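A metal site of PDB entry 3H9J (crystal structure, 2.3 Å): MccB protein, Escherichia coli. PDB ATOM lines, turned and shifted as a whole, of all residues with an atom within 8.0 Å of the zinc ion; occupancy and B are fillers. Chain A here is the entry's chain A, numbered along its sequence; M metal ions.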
ATOM      1  N   ASN A 227      17.966 -12.536   6.943  1.00  0.00           N
ATOM      2  CA  ASN A 227      18.728 -12.897   5.759  1.00  0.00           C
ATOM      3  C   ASN A 227      18.902 -14.413   5.601  1.00  0.00           C
ATOM      4  O   ASN A 227      18.579 -14.956   4.551  1.00  0.00           O
ATOM      5  CB  ASN A 227      20.080 -12.185   5.748  1.00  0.00           C
ATOM      6  CG  ASN A 227      20.854 -12.449   4.475  1.00  0.00           C
ATOM      7  OD1 ASN A 227      20.500 -11.955   3.409  1.00  0.00           O
ATOM      8  ND2 ASN A 227      21.906 -13.241   4.590  1.00  0.00           N
ATOM      9  N   VAL A 231      17.109 -16.428   2.574  1.00  0.00           N
ATOM     10  CA  VAL A 231      17.907 -17.237   1.642  1.00  0.00           C
ATOM     11  C   VAL A 231      17.357 -18.649   1.543  1.00  0.00           C
ATOM     12  O   VAL A 231      17.172 -19.176   0.449  1.00  0.00           O
ATOM     13  CB  VAL A 231      19.430 -17.243   1.992  1.00  0.00           C
ATOM     14  CG1 VAL A 231      20.167 -18.370   1.266  1.00  0.00           C
ATOM     15  CG2 VAL A 231      20.055 -15.892   1.656  1.00  0.00           C
ATOM     16  N   TYR A 253      17.334  -8.020  -1.392  1.00  0.00           N
ATOM     17  CA  TYR A 253      17.677  -9.398  -1.699  1.00  0.00           C
ATOM     18  C   TYR A 253      16.666 -10.049  -2.629  1.00  0.00           C
ATOM     19  O   TYR A 253      15.488 -10.129  -2.326  1.00  0.00           O
ATOM     20  CB  TYR A 253      17.865 -10.210  -0.412  1.00  0.00           C
ATOM     21  CG  TYR A 253      18.098 -11.683  -0.665  1.00  0.00           C
ATOM     22  CD1 TYR A 253      19.311 -12.134  -1.163  1.00  0.00           C
ATOM     23  CD2 TYR A 253      17.091 -12.614  -0.408  1.00  0.00           C
ATOM     24  CE1 TYR A 253      19.515 -13.482  -1.417  1.00  0.00           C
ATOM     25  CE2 TYR A 253      17.290 -13.967  -0.650  1.00  0.00           C
ATOM     26  CZ  TYR A 253      18.500 -14.384  -1.161  1.00  0.00           C
ATOM     27  OH  TYR A 253      18.711 -15.717  -1.405  1.00  0.00           O
ATOM     28  N   THR A 258      20.890 -11.853  -6.918  1.00  0.00           N
ATOM     29  CA  THR A 258      21.547 -10.798  -6.142  1.00  0.00           C
ATOM     30  C   THR A 258      22.345 -11.406  -4.975  1.00  0.00           C
ATOM     31  O   THR A 258      22.119 -12.547  -4.616  1.00  0.00           O
ATOM     32  CB  THR A 258      20.482  -9.760  -5.614  1.00  0.00           C
ATOM     33  OG1 THR A 258      20.995  -8.432  -5.723  1.00  0.00           O
ATOM     34  CG2 THR A 258      20.088 -10.034  -4.166  1.00  0.00           C
ATOM     35  N   GLY A 259      23.273 -10.653  -4.410  1.00  0.00           N
ATOM     36  CA  GLY A 259      23.984 -11.093  -3.212  1.00  0.00           C
ATOM     37  C   GLY A 259      23.165 -10.908  -1.940  1.00  0.00           C
ATOM     38  O   GLY A 259      22.241 -10.088  -1.901  1.00  0.00           O
ATOM     39  N   CYS A 260      23.503 -11.674  -0.904  1.00  0.00           N
ATOM     40  CA  CYS A 260      22.798 -11.578   0.372  1.00  0.00           C
ATOM     41  C   CYS A 260      23.589 -10.695   1.345  1.00  0.00           C
ATOM     42  O   CYS A 260      24.683 -10.220   1.020  1.00  0.00           O
ATOM     43  CB  CYS A 260      22.510 -12.960   0.957  1.00  0.00           C
ATOM     44  SG  CYS A 260      23.806 -13.729   1.969  1.00  0.00           S
ATOM     45  N   TYR A 261      23.020 -10.505   2.530  1.00  0.00           N
ATOM     46  CA  TYR A 261      23.572  -9.602   3.537  1.00  0.00           C
ATOM     47  C   TYR A 261      24.974  -9.993   4.040  1.00  0.00           C
ATOM     48  O   TYR A 261      25.780  -9.114   4.355  1.00  0.00           O
ATOM     49  CB  TYR A 261      22.604  -9.510   4.719  1.00  0.00           C
ATOM     50  CG  TYR A 261      22.875  -8.382   5.695  1.00  0.00           C
ATOM     51  CD1 TYR A 261      22.424  -7.080   5.431  1.00  0.00           C
ATOM     52  CD2 TYR A 261      23.572  -8.609   6.877  1.00  0.00           C
ATOM     53  CE1 TYR A 261      22.674  -6.041   6.321  1.00  0.00           C
ATOM     54  CE2 TYR A 261      23.825  -7.575   7.775  1.00  0.00           C
ATOM     55  CZ  TYR A 261      23.372  -6.300   7.492  1.00  0.00           C
ATOM     56  OH  TYR A 261      23.599  -5.278   8.365  1.00  0.00           O
ATOM     57  N   GLU A 262      25.236 -11.296   4.088  1.00  0.00           N
ATOM     58  CA  GLU A 262      26.484 -11.860   4.641  1.00  0.00           C
ATOM     59  C   GLU A 262      27.617 -12.035   3.606  1.00  0.00           C
ATOM     60  O   GLU A 262      28.753 -12.336   3.982  1.00  0.00           O
ATOM     61  CB  GLU A 262      26.194 -13.201   5.324  1.00  0.00           C
ATOM     62  CG  GLU A 262      25.640 -13.118   6.766  1.00  0.00           C
ATOM     63  CD  GLU A 262      24.114 -12.976   6.839  1.00  0.00           C
ATOM     64  OE1 GLU A 262      23.406 -13.963   7.142  1.00  0.00           O
ATOM     65  OE2 GLU A 262      23.612 -11.858   6.588  1.00  0.00           O
ATOM     66  N   CYS A 263      27.314 -11.826   2.314  1.00  0.00           N
ATOM     67  CA  CYS A 263      28.237 -12.057   1.191  1.00  0.00           C
ATOM     68  C   CYS A 263      29.586 -11.327   1.235  1.00  0.00           C
ATOM     69  O   CYS A 263      30.612 -11.882   0.840  1.00  0.00           O
ATOM     70  CB  CYS A 263      27.572 -11.709  -0.137  1.00  0.00           C
ATOM     71  SG  CYS A 263      26.830 -13.085  -0.977  1.00  0.00           S
ATOM     72  N   GLN A 264      29.556 -10.077   1.699  1.00  0.00           N
ATOM     73  CA  GLN A 264      30.727  -9.214   1.627  1.00  0.00           C
ATOM     74  C   GLN A 264      31.311  -8.873   2.998  1.00  0.00           C
ATOM     75  O   GLN A 264      32.118  -7.946   3.124  1.00  0.00           O
ATOM     76  CB  GLN A 264      30.403  -7.946   0.822  1.00  0.00           C
ATOM     77  CG  GLN A 264      29.978  -8.208  -0.632  1.00  0.00           C
ATOM     78  CD  GLN A 264      31.114  -8.739  -1.505  1.00  0.00           C
ATOM     79  OE1 GLN A 264      32.286  -8.393  -1.310  1.00  0.00           O
ATOM     80  NE2 GLN A 264      30.774  -9.602  -2.461  1.00  0.00           N
ATOM     81  N   MET A 340      27.416  -5.084  -1.801  1.00  0.00           N
ATOM     82  CA  MET A 340      26.818  -6.291  -1.247  1.00  0.00           C
ATOM     83  C   MET A 340      26.468  -7.274  -2.371  1.00  0.00           C
ATOM     84  O   MET A 340      25.420  -7.935  -2.353  1.00  0.00           O
ATOM     85  CB  MET A 340      25.586  -5.977  -0.397  1.00  0.00           C
ATOM     86  CG  MET A 340      25.831  -4.982   0.740  1.00  0.00           C
ATOM     87  SD  MET A 340      24.883  -5.282   2.237  1.00  0.00           S
ATOM     88  CE  MET A 340      23.939  -6.717   1.792  1.00  0.00           C
ATOM     89  N   GLY A 341      27.365  -7.361  -3.361  1.00  0.00           N
ATOM     90  CA  GLY A 341      27.216  -8.284  -4.482  1.00  0.00           C
ATOM     91  C   GLY A 341      27.429  -9.729  -4.072  1.00  0.00           C
ATOM     92  O   GLY A 341      27.972  -9.997  -3.004  1.00  0.00           O
ATOM     93  N   ARG A 342      27.006 -10.650  -4.933  1.00  0.00           N
ATOM     94  CA  ARG A 342      27.106 -12.091  -4.658  1.00  0.00           C
ATOM     95  C   ARG A 342      28.540 -12.541  -4.478  1.00  0.00           C
ATOM     96  O   ARG A 342      29.422 -12.149  -5.242  1.00  0.00           O
ATOM     97  CB  ARG A 342      26.409 -12.920  -5.747  1.00  0.00           C
ATOM     98  CG  ARG A 342      25.998 -14.313  -5.267  1.00  0.00           C
ATOM     99  CD  ARG A 342      25.138 -15.101  -6.244  1.00  0.00           C
ATOM    100  NE  ARG A 342      24.490 -16.195  -5.530  1.00  0.00           N
ATOM    101  CZ  ARG A 342      24.041 -17.339  -6.074  1.00  0.00           C
ATOM    102  NH1 ARG A 342      24.160 -17.577  -7.377  1.00  0.00           N
ATOM    103  NH2 ARG A 342      23.477 -18.240  -5.287  1.00  0.00           N
ATOM    104  N   SER A 343      28.762 -13.347  -3.438  1.00  0.00           N
ATOM    105  CA  SER A 343      30.026 -14.043  -3.218  1.00  0.00           C
ATOM    106  C   SER A 343      29.805 -15.553  -3.288  1.00  0.00           C
ATOM    107  O   SER A 343      29.039 -16.108  -2.498  1.00  0.00           O
ATOM    108  CB  SER A 343      30.636 -13.661  -1.852  1.00  0.00           C
ATOM    109  OG  SER A 343      31.648 -14.581  -1.448  1.00  0.00           O
ATOM    110  N   PRO A 344      30.480 -16.214  -4.255  1.00  0.00           N
ATOM    111  CA  PRO A 344      30.336 -17.652  -4.461  1.00  0.00           C
ATOM    112  C   PRO A 344      30.807 -18.430  -3.250  1.00  0.00           C
ATOM    113  O   PRO A 344      30.458 -19.605  -3.078  1.00  0.00           O
ATOM    114  CB  PRO A 344      31.279 -17.931  -5.643  1.00  0.00           C
ATOM    115  CG  PRO A 344      31.490 -16.625  -6.294  1.00  0.00           C
ATOM    116  CD  PRO A 344      31.436 -15.614  -5.195  1.00  0.00           C
ATOM    117  N   VAL A 345      31.586 -17.753  -2.403  1.00  0.00           N
ATOM    118  CA  VAL A 345      32.215 -18.350  -1.238  1.00  0.00           C
ATOM    119  C   VAL A 345      31.461 -17.978   0.070  1.00  0.00           C
ATOM    120  O   VAL A 345      31.909 -18.309   1.168  1.00  0.00           O
ATOM    121  CB  VAL A 345      33.755 -18.002  -1.207  1.00  0.00           C
ATOM    122  CG1 VAL A 345      34.439 -18.511   0.043  1.00  0.00           C
ATOM    123  CG2 VAL A 345      34.447 -18.613  -2.421  1.00  0.00           C
ATOM    124  N   CYS A 346      30.301 -17.325  -0.067  1.00  0.00           N
ATOM    125  CA  CYS A 346      29.456 -16.974   1.090  1.00  0.00           C
ATOM    126  C   CYS A 346      28.937 -18.226   1.789  1.00  0.00           C
ATOM    127  O   CYS A 346      28.542 -19.187   1.124  1.00  0.00           O
ATOM    128  CB  CYS A 346      28.269 -16.104   0.667  1.00  0.00           C
ATOM    129  SG  CYS A 346      27.108 -15.734   2.021  1.00  0.00           S
ATOM    130  N   SER A 347      28.927 -18.196   3.113  1.00  0.00           N
ATOM    131  CA  SER A 347      28.541 -19.370   3.897  1.00  0.00           C
ATOM    132  C   SER A 347      27.022 -19.531   4.040  1.00  0.00           C
ATOM    133  O   SER A 347      26.540 -20.591   4.407  1.00  0.00           O
ATOM    134  CB  SER A 347      29.197 -19.344   5.289  1.00  0.00           C
ATOM    135  OG  SER A 347      28.637 -18.334   6.105  1.00  0.00           O
ATOM    136  N   VAL A 348      26.295 -18.458   3.714  1.00  0.00           N
ATOM    137  CA  VAL A 348      24.837 -18.452   3.801  1.00  0.00           C
ATOM    138  C   VAL A 348      24.189 -18.854   2.476  1.00  0.00           C
ATOM    139  O   VAL A 348      23.426 -19.819   2.422  1.00  0.00           O
ATOM    140  CB  VAL A 348      24.290 -17.079   4.306  1.00  0.00           C
ATOM    141  CG1 VAL A 348      22.772 -17.047   4.266  1.00  0.00           C
ATOM    142  CG2 VAL A 348      24.796 -16.787   5.712  1.00  0.00           C
ATOM    143  N   CYS A 349      24.507 -18.127   1.406  1.00  0.00           N
ATOM    144  CA  CYS A 349      23.865 -18.369   0.120  1.00  0.00           C
ATOM    145  C   CYS A 349      24.768 -19.028  -0.913  1.00  0.00           C
ATOM    146  O   CYS A 349      24.340 -19.281  -2.042  1.00  0.00           O
ATOM    147  CB  CYS A 349      23.284 -17.057  -0.426  1.00  0.00           C
ATOM    148  SG  CYS A 349      24.491 -15.836  -1.007  1.00  0.00           S
ATOM    149  N   GLY A 350      26.003 -19.349  -0.513  1.00  0.00           N
ATOM    150  CA  GLY A 350      27.063 -19.728  -1.462  1.00  0.00           C
ATOM    151  C   GLY A 350      27.053 -21.132  -2.054  1.00  0.00           C
ATOM    152  O   GLY A 350      26.049 -21.577  -2.604  1.00  0.00           O
HETATM  153 ZN    ZN M   1      25.505 -14.622   0.563  1.00  0.00          ZN
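The zinc ion is bound by SG of Cys 349 (2.2 Å), SG of Cys 260 (2.4 Å), SG of Cys 346 (2.4 Å) and SG of Cys 263 (2.5 Å).
The zinc ion has four donor atoms within binding distance.
Within 4 Å of the zinc ion: Cys 260, Cys 263, Cys 346 and Cys 349.
SG of Cys 260 lies close to ND2 of Asn 227, 3.3 Å away.
The side-chain hydroxyl (OG) of Ser 343 lies within hydrogen-bond range of the backbone NH (N) of Cys 346 (3.4 Å).
The side-chain sulfur (SG) of Cys 263 sits close to the backbone NH (N) of Ser 343 (3.1 Å).
The backbone NH (N) of Val 348 lies close to the side-chain sulfur (SG) of Cys 346.
N of Glu 262 sits close to SG of Cys 260, 3.5 Å away.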
